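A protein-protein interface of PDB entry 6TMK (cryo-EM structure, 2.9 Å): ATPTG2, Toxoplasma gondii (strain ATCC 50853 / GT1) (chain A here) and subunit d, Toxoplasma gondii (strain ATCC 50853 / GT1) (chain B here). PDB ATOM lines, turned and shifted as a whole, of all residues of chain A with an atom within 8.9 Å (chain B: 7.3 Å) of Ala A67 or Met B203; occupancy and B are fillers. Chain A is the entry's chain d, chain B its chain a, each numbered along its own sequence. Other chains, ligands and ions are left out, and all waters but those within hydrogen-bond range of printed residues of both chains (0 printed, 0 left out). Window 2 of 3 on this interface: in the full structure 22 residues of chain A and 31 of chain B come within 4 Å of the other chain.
Of the printed residues of chain B, Tyr A63 touches Asn B207.
Of chain B, only Trp B199, Arg B202 and Met B203 come within 4 Å of Ala A67.
Of the printed residues of chain B, Thr A68 touches Trp B199 (3.8 Å).
Tyr A71 touches none of the printed residues of chain B.
Arg A77 touches none of the printed residues of chain B.
Of the printed residues of chain A, Trp B199 touches His A66, Ala A67 and Thr A68.
Met B203 touches just these residues of chain A: Glu A65 (3.3 Å) and Ala A67 (3.9 Å).
No residue of chain A comes within 4 Å of Gly B204.
Of the printed residues of chain A, Asn B207 touches Tyr A62 (2.6 Å), Tyr A63 (3.6 Å) and Gly A64 (3.0 Å).
The nearest printed residue of chain B that does not touch Ala A67 is Ala B198 (7.7 Å).
Of the 12 printed residues of chain A, 7 touch a printed residue of chain B.
Hydrophobic or aromatic side chains of chain A within 4 Å of the printed part of chain B: Tyr A62, Tyr A63, His A66 and Ala A67.
Along chain A the printed residues that touch a printed residue of chain B span positions 62 to 68.
Printed residues of chain B that touch a printed residue of chain A: Trp B199, Arg B202, Met B203 and Asn B207.
Hydrophobic or aromatic side chains of chain B within 4 Å of the printed part of chain A: Trp B199 and Met B203.
Among the printed residues, 9 pairs touch across the chains.
A ring nitrogen (ND1) of His A66 sits close to the backbone NH (N) of Thr A68 (3.4 Å).
A ring nitrogen (ND1) of His A66 sits at hydrogen-bond distance from the backbone NH (N) of Tyr A69, 3.3 Å away.
The backbone carbonyl oxygen (O) of Met B203 sits at hydrogen-bond distance from the side-chain amide nitrogen (ND2) of Asn B207, 3.4 Å away.
Among the printed residues, pairs that only touch across the chains: Glu A65 with Met B203 (3.3 Å), His A66 with Trp B199 (3.4 Å), Tyr A63 with Asn B207 (3.6 Å), Ala A67 with Trp B199 (3.6 Å), Ala A67 with Arg B202 (3.6 Å), Thr A68 with Trp B199 (3.8 Å) and Ala A67 with Met B203 (3.9 Å).
The backbone carbonyl oxygen of Asn B207 sits at hydrogen-bond distance from the side-chain hydroxyl of Tyr A62 (2.6 Å).
The side-chain amide oxygen of Asn B207 sits at hydrogen-bond distance from the backbone NH of Gly A64 (3.0 Å).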
ATOM      1  N   TYR A  62      21.877  17.084  -8.568  1.00  0.00           N
ATOM      2  CA  TYR A  62      22.192  18.451  -8.182  1.00  0.00           C
ATOM      3  C   TYR A  62      22.391  19.368  -9.376  1.00  0.00           C
ATOM      4  O   TYR A  62      21.836  20.468  -9.415  1.00  0.00           O
ATOM      5  CB  TYR A  62      23.452  18.487  -7.312  1.00  0.00           C
ATOM      6  CG  TYR A  62      24.038  19.869  -7.214  1.00  0.00           C
ATOM      7  CD1 TYR A  62      23.415  20.851  -6.471  1.00  0.00           C
ATOM      8  CD2 TYR A  62      25.198  20.198  -7.884  1.00  0.00           C
ATOM      9  CE1 TYR A  62      23.938  22.118  -6.389  1.00  0.00           C
ATOM     10  CE2 TYR A  62      25.725  21.461  -7.809  1.00  0.00           C
ATOM     11  CZ  TYR A  62      25.091  22.418  -7.064  1.00  0.00           C
ATOM     12  OH  TYR A  62      25.619  23.680  -6.987  1.00  0.00           O
ATOM     13  N   TYR A  63      23.175  18.936 -10.356  1.00  0.00           N
ATOM     14  CA  TYR A  63      23.650  19.848 -11.383  1.00  0.00           C
ATOM     15  C   TYR A  63      22.543  20.197 -12.363  1.00  0.00           C
ATOM     16  O   TYR A  63      21.697  19.366 -12.700  1.00  0.00           O
ATOM     17  CB  TYR A  63      24.826  19.232 -12.131  1.00  0.00           C
ATOM     18  CG  TYR A  63      26.107  19.249 -11.347  1.00  0.00           C
ATOM     19  CD1 TYR A  63      26.779  20.431 -11.115  1.00  0.00           C
ATOM     20  CD2 TYR A  63      26.636  18.085 -10.829  1.00  0.00           C
ATOM     21  CE1 TYR A  63      27.944  20.453 -10.392  1.00  0.00           C
ATOM     22  CE2 TYR A  63      27.801  18.096 -10.106  1.00  0.00           C
ATOM     23  CZ  TYR A  63      28.452  19.284  -9.892  1.00  0.00           C
ATOM     24  OH  TYR A  63      29.615  19.313  -9.170  1.00  0.00           O
ATOM     25  N   GLY A  64      22.562  21.445 -12.821  1.00  0.00           N
ATOM     26  CA  GLY A  64      21.582  21.887 -13.782  1.00  0.00           C
ATOM     27  C   GLY A  64      21.821  21.293 -15.155  1.00  0.00           C
ATOM     28  O   GLY A  64      22.946  20.981 -15.542  1.00  0.00           O
ATOM     29  N   GLU A  65      20.735  21.142 -15.902  1.00  0.00           N
ATOM     30  CA  GLU A  65      20.819  20.541 -17.217  1.00  0.00           C
ATOM     31  C   GLU A  65      21.597  21.437 -18.175  1.00  0.00           C
ATOM     32  O   GLU A  65      21.996  22.558 -17.850  1.00  0.00           O
ATOM     33  CB  GLU A  65      19.425  20.245 -17.767  1.00  0.00           C
ATOM     34  CG  GLU A  65      18.528  21.448 -17.993  1.00  0.00           C
ATOM     35  CD  GLU A  65      17.722  21.808 -16.763  1.00  0.00           C
ATOM     36  OE1 GLU A  65      18.105  21.392 -15.651  1.00  0.00           O
ATOM     37  OE2 GLU A  65      16.690  22.494 -16.909  1.00  0.00           O
ATOM     38  N   HIS A  66      21.813  20.910 -19.374  1.00  0.00           N
ATOM     39  CA  HIS A  66      22.408  21.681 -20.451  1.00  0.00           C
ATOM     40  C   HIS A  66      21.645  22.974 -20.692  1.00  0.00           C
ATOM     41  O   HIS A  66      20.418  23.019 -20.600  1.00  0.00           O
ATOM     42  CB  HIS A  66      22.406  20.842 -21.723  1.00  0.00           C
ATOM     43  CG  HIS A  66      23.565  21.095 -22.629  1.00  0.00           C
ATOM     44  ND1 HIS A  66      23.569  22.107 -23.563  1.00  0.00           N
ATOM     45  CD2 HIS A  66      24.746  20.454 -22.764  1.00  0.00           C
ATOM     46  CE1 HIS A  66      24.709  22.084 -24.225  1.00  0.00           C
ATOM     47  NE2 HIS A  66      25.442  21.092 -23.758  1.00  0.00           N
ATOM     48  N   ALA A  67      22.388  24.030 -21.014  1.00  0.00           N
ATOM     49  CA  ALA A  67      21.776  25.339 -21.168  1.00  0.00           C
ATOM     50  C   ALA A  67      21.017  25.450 -22.483  1.00  0.00           C
ATOM     51  O   ALA A  67      19.963  26.091 -22.542  1.00  0.00           O
ATOM     52  CB  ALA A  67      22.845  26.424 -21.080  1.00  0.00           C
ATOM     53  N   THR A  68      21.535  24.837 -23.545  1.00  0.00           N
ATOM     54  CA  THR A  68      20.983  25.006 -24.879  1.00  0.00           C
ATOM     55  C   THR A  68      20.272  23.773 -25.411  1.00  0.00           C
ATOM     56  O   THR A  68      19.369  23.911 -26.237  1.00  0.00           O
ATOM     57  CB  THR A  68      22.089  25.415 -25.859  1.00  0.00           C
ATOM     58  OG1 THR A  68      21.575  25.450 -27.194  1.00  0.00           O
ATOM     59  CG2 THR A  68      23.234  24.474 -25.796  1.00  0.00           C
ATOM     60  N   TYR A  69      20.654  22.579 -24.971  1.00  0.00           N
ATOM     61  CA  TYR A  69      19.962  21.344 -25.330  1.00  0.00           C
ATOM     62  C   TYR A  69      19.359  20.781 -24.051  1.00  0.00           C
ATOM     63  O   TYR A  69      19.904  19.870 -23.430  1.00  0.00           O
ATOM     64  CB  TYR A  69      20.890  20.347 -25.988  1.00  0.00           C
ATOM     65  CG  TYR A  69      21.582  20.876 -27.209  1.00  0.00           C
ATOM     66  CD1 TYR A  69      20.859  21.356 -28.281  1.00  0.00           C
ATOM     67  CD2 TYR A  69      22.959  20.891 -27.292  1.00  0.00           C
ATOM     68  CE1 TYR A  69      21.486  21.843 -29.392  1.00  0.00           C
ATOM     69  CE2 TYR A  69      23.592  21.375 -28.401  1.00  0.00           C
ATOM     70  CZ  TYR A  69      22.852  21.851 -29.449  1.00  0.00           C
ATOM     71  OH  TYR A  69      23.485  22.339 -30.563  1.00  0.00           O
ATOM     72  N   ASN A  70      18.209  21.312 -23.677  1.00  0.00           N
ATOM     73  CA  ASN A  70      17.564  20.952 -22.431  1.00  0.00           C
ATOM     74  C   ASN A  70      16.307  20.130 -22.691  1.00  0.00           C
ATOM     75  O   ASN A  70      15.860  19.934 -23.830  1.00  0.00           O
ATOM     76  CB  ASN A  70      17.259  22.202 -21.607  1.00  0.00           C
ATOM     77  CG  ASN A  70      16.356  23.170 -22.319  1.00  0.00           C
ATOM     78  OD1 ASN A  70      15.190  22.883 -22.579  1.00  0.00           O
ATOM     79  ND2 ASN A  70      16.886  24.333 -22.632  1.00  0.00           N
ATOM     80  N   TYR A  71      15.719  19.680 -21.585  1.00  0.00           N
ATOM     81  CA  TYR A  71      14.649  18.698 -21.647  1.00  0.00           C
ATOM     82  C   TYR A  71      13.437  19.269 -22.361  1.00  0.00           C
ATOM     83  O   TYR A  71      12.873  18.636 -23.261  1.00  0.00           O
ATOM     84  CB  TYR A  71      14.276  18.259 -20.235  1.00  0.00           C
ATOM     85  CG  TYR A  71      15.447  17.919 -19.350  1.00  0.00           C
ATOM     86  CD1 TYR A  71      16.432  17.045 -19.767  1.00  0.00           C
ATOM     87  CD2 TYR A  71      15.566  18.481 -18.095  1.00  0.00           C
ATOM     88  CE1 TYR A  71      17.498  16.743 -18.953  1.00  0.00           C
ATOM     89  CE2 TYR A  71      16.623  18.183 -17.281  1.00  0.00           C
ATOM     90  CZ  TYR A  71      17.585  17.315 -17.711  1.00  0.00           C
ATOM     91  OH  TYR A  71      18.639  17.029 -16.883  1.00  0.00           O
ATOM     92  N   VAL A  73      13.150  21.885 -24.426  1.00  0.00           N
ATOM     93  CA  VAL A  73      13.303  22.281 -25.816  1.00  0.00           C
ATOM     94  C   VAL A  73      13.371  21.047 -26.702  1.00  0.00           C
ATOM     95  O   VAL A  73      12.775  21.014 -27.785  1.00  0.00           O
ATOM     96  CB  VAL A  73      14.531  23.194 -25.986  1.00  0.00           C
ATOM     97  CG1 VAL A  73      15.808  22.410 -25.952  1.00  0.00           C
ATOM     98  CG2 VAL A  73      14.422  24.010 -27.241  1.00  0.00           C
ATOM     99  N   ARG A  77      10.464  20.293 -29.464  1.00  0.00           N
ATOM    100  CA  ARG A  77      10.904  20.015 -30.821  1.00  0.00           C
ATOM    101  C   ARG A  77      10.407  18.660 -31.301  1.00  0.00           C
ATOM    102  O   ARG A  77      10.159  18.480 -32.498  1.00  0.00           O
ATOM    103  CB  ARG A  77      12.420  20.106 -30.904  1.00  0.00           C
ATOM    104  CG  ARG A  77      12.909  21.522 -30.857  1.00  0.00           C
ATOM    105  CD  ARG A  77      14.397  21.634 -30.807  1.00  0.00           C
ATOM    106  NE  ARG A  77      14.807  22.989 -30.479  1.00  0.00           N
ATOM    107  CZ  ARG A  77      16.065  23.385 -30.358  1.00  0.00           C
ATOM    108  NH1 ARG A  77      17.051  22.538 -30.549  1.00  0.00           N
ATOM    109  NH2 ARG A  77      16.334  24.640 -30.061  1.00  0.00           N
ATOM    110  N   GLN B 197      32.629  30.654 -24.383  1.00  0.00           N
ATOM    111  CA  GLN B 197      33.097  31.167 -23.103  1.00  0.00           C
ATOM    112  C   GLN B 197      31.940  31.651 -22.247  1.00  0.00           C
ATOM    113  O   GLN B 197      31.924  31.433 -21.030  1.00  0.00           O
ATOM    114  CB  GLN B 197      34.101  32.290 -23.328  1.00  0.00           C
ATOM    115  CG  GLN B 197      35.369  31.833 -23.999  1.00  0.00           C
ATOM    116  CD  GLN B 197      36.122  30.809 -23.175  1.00  0.00           C
ATOM    117  OE1 GLN B 197      36.043  30.802 -21.947  1.00  0.00           O
ATOM    118  NE2 GLN B 197      36.840  29.925 -23.850  1.00  0.00           N
ATOM    119  N   ALA B 198      30.966  32.321 -22.861  1.00  0.00           N
ATOM    120  CA  ALA B 198      29.775  32.733 -22.131  1.00  0.00           C
ATOM    121  C   ALA B 198      29.029  31.528 -21.577  1.00  0.00           C
ATOM    122  O   ALA B 198      28.567  31.548 -20.433  1.00  0.00           O
ATOM    123  CB  ALA B 198      28.875  33.556 -23.043  1.00  0.00           C
ATOM    124  N   TRP B 199      28.890  30.479 -22.385  1.00  0.00           N
ATOM    125  CA  TRP B 199      28.255  29.247 -21.933  1.00  0.00           C
ATOM    126  C   TRP B 199      28.934  28.714 -20.683  1.00  0.00           C
ATOM    127  O   TRP B 199      28.280  28.430 -19.669  1.00  0.00           O
ATOM    128  CB  TRP B 199      28.322  28.221 -23.063  1.00  0.00           C
ATOM    129  CG  TRP B 199      27.424  27.048 -22.938  1.00  0.00           C
ATOM    130  CD1 TRP B 199      26.202  26.903 -23.506  1.00  0.00           C
ATOM    131  CD2 TRP B 199      27.678  25.838 -22.222  1.00  0.00           C
ATOM    132  NE1 TRP B 199      25.671  25.686 -23.186  1.00  0.00           N
ATOM    133  CE2 TRP B 199      26.558  25.010 -22.396  1.00  0.00           C
ATOM    134  CE3 TRP B 199      28.741  25.375 -21.449  1.00  0.00           C
ATOM    135  CZ2 TRP B 199      26.470  23.752 -21.822  1.00  0.00           C
ATOM    136  CZ3 TRP B 199      28.648  24.129 -20.882  1.00  0.00           C
ATOM    137  CH2 TRP B 199      27.524  23.330 -21.072  1.00  0.00           C
ATOM    138  N   HIS B 200      30.256  28.574 -20.740  1.00  0.00           N
ATOM    139  CA  HIS B 200      30.985  28.013 -19.611  1.00  0.00           C
ATOM    140  C   HIS B 200      30.899  28.908 -18.385  1.00  0.00           C
ATOM    141  O   HIS B 200      30.727  28.417 -17.264  1.00  0.00           O
ATOM    142  CB  HIS B 200      32.436  27.765 -20.002  1.00  0.00           C
ATOM    143  CG  HIS B 200      32.628  26.527 -20.814  1.00  0.00           C
ATOM    144  ND1 HIS B 200      32.481  25.264 -20.284  1.00  0.00           N
ATOM    145  CD2 HIS B 200      32.941  26.354 -22.118  1.00  0.00           C
ATOM    146  CE1 HIS B 200      32.701  24.366 -21.227  1.00  0.00           C
ATOM    147  NE2 HIS B 200      32.982  25.002 -22.349  1.00  0.00           N
ATOM    148  N   SER B 201      30.993  30.223 -18.571  1.00  0.00           N
ATOM    149  CA  SER B 201      30.926  31.131 -17.433  1.00  0.00           C
ATOM    150  C   SER B 201      29.547  31.109 -16.792  1.00  0.00           C
ATOM    151  O   SER B 201      29.427  31.128 -15.563  1.00  0.00           O
ATOM    152  CB  SER B 201      31.295  32.542 -17.877  1.00  0.00           C
ATOM    153  OG  SER B 201      30.313  33.071 -18.742  1.00  0.00           O
ATOM    154  N   ARG B 202      28.496  31.064 -17.608  1.00  0.00           N
ATOM    155  CA  ARG B 202      27.138  30.992 -17.086  1.00  0.00           C
ATOM    156  C   ARG B 202      26.941  29.722 -16.276  1.00  0.00           C
ATOM    157  O   ARG B 202      26.443  29.759 -15.143  1.00  0.00           O
ATOM    158  CB  ARG B 202      26.140  31.053 -18.237  1.00  0.00           C
ATOM    159  CG  ARG B 202      26.061  32.402 -18.893  1.00  0.00           C
ATOM    160  CD  ARG B 202      25.574  32.296 -20.321  1.00  0.00           C
ATOM    161  NE  ARG B 202      24.454  31.375 -20.464  1.00  0.00           N
ATOM    162  CZ  ARG B 202      24.103  30.810 -21.612  1.00  0.00           C
ATOM    163  NH1 ARG B 202      24.781  31.063 -22.718  1.00  0.00           N
ATOM    164  NH2 ARG B 202      23.066  29.993 -21.657  1.00  0.00           N
ATOM    165  N   MET B 203      27.326  28.582 -16.845  1.00  0.00           N
ATOM    166  CA  MET B 203      27.128  27.321 -16.146  1.00  0.00           C
ATOM    167  C   MET B 203      27.951  27.272 -14.868  1.00  0.00           C
ATOM    168  O   MET B 203      27.487  26.759 -13.844  1.00  0.00           O
ATOM    169  CB  MET B 203      27.489  26.160 -17.062  1.00  0.00           C
ATOM    170  CG  MET B 203      26.599  26.054 -18.274  1.00  0.00           C
ATOM    171  SD  MET B 203      24.889  25.687 -17.870  1.00  0.00           S
ATOM    172  CE  MET B 203      25.018  23.930 -17.610  1.00  0.00           C
ATOM    173  N   GLY B 204      29.170  27.802 -14.903  1.00  0.00           N
ATOM    174  CA  GLY B 204      29.973  27.845 -13.699  1.00  0.00           C
ATOM    175  C   GLY B 204      29.355  28.713 -12.625  1.00  0.00           C
ATOM    176  O   GLY B 204      29.249  28.308 -11.468  1.00  0.00           O
ATOM    177  N   LYS B 205      28.933  29.921 -12.991  1.00  0.00           N
ATOM    178  CA  LYS B 205      28.311  30.798 -12.012  1.00  0.00           C
ATOM    179  C   LYS B 205      27.059  30.176 -11.421  1.00  0.00           C
ATOM    180  O   LYS B 205      26.759  30.386 -10.242  1.00  0.00           O
ATOM    181  CB  LYS B 205      27.973  32.142 -12.647  1.00  0.00           C
ATOM    182  CG  LYS B 205      27.563  33.199 -11.646  1.00  0.00           C
ATOM    183  CD  LYS B 205      27.366  34.546 -12.299  1.00  0.00           C
ATOM    184  CE  LYS B 205      26.501  35.451 -11.435  1.00  0.00           C
ATOM    185  NZ  LYS B 205      26.956  35.496 -10.011  1.00  0.00           N
ATOM    186  N   PHE B 206      26.319  29.408 -12.215  1.00  0.00           N
ATOM    187  CA  PHE B 206      25.097  28.807 -11.701  1.00  0.00           C
ATOM    188  C   PHE B 206      25.391  27.629 -10.779  1.00  0.00           C
ATOM    189  O   PHE B 206      24.817  27.528  -9.691  1.00  0.00           O
ATOM    190  CB  PHE B 206      24.198  28.373 -12.857  1.00  0.00           C
ATOM    191  CG  PHE B 206      22.887  27.809 -12.418  1.00  0.00           C
ATOM    192  CD1 PHE B 206      22.595  26.475 -12.603  1.00  0.00           C
ATOM    193  CD2 PHE B 206      21.946  28.613 -11.811  1.00  0.00           C
ATOM    194  CE1 PHE B 206      21.394  25.960 -12.192  1.00  0.00           C
ATOM    195  CE2 PHE B 206      20.751  28.102 -11.404  1.00  0.00           C
ATOM    196  CZ  PHE B 206      20.472  26.773 -11.592  1.00  0.00           C
ATOM    197  N   ASN B 207      26.283  26.730 -11.191  1.00  0.00           N
ATOM    198  CA  ASN B 207      26.440  25.447 -10.522  1.00  0.00           C
ATOM    199  C   ASN B 207      27.551  25.410  -9.482  1.00  0.00           C
ATOM    200  O   ASN B 207      27.481  24.598  -8.555  1.00  0.00           O
ATOM    201  CB  ASN B 207      26.718  24.359 -11.559  1.00  0.00           C
ATOM    202  CG  ASN B 207      25.468  23.885 -12.252  1.00  0.00           C
ATOM    203  OD1 ASN B 207      24.588  23.287 -11.639  1.00  0.00           O
ATOM    204  ND2 ASN B 207      25.382  24.154 -13.544  1.00  0.00           N
ATOM    205  N   ASP B 208      28.569  26.251  -9.606  1.00  0.00           N
ATOM    206  CA  ASP B 208      29.755  26.109  -8.778  1.00  0.00           C
ATOM    207  C   ASP B 208      29.487  26.498  -7.330  1.00  0.00           C
ATOM    208  O   ASP B 208      28.606  27.306  -7.023  1.00  0.00           O
ATOM    209  CB  ASP B 208      30.891  26.964  -9.331  1.00  0.00           C
ATOM    210  CG  ASP B 208      31.453  26.420 -10.628  1.00  0.00           C
ATOM    211  OD1 ASP B 208      32.232  27.143 -11.285  1.00  0.00           O
ATOM    212  OD2 ASP B 208      31.120  25.273 -10.992  1.00  0.00           O
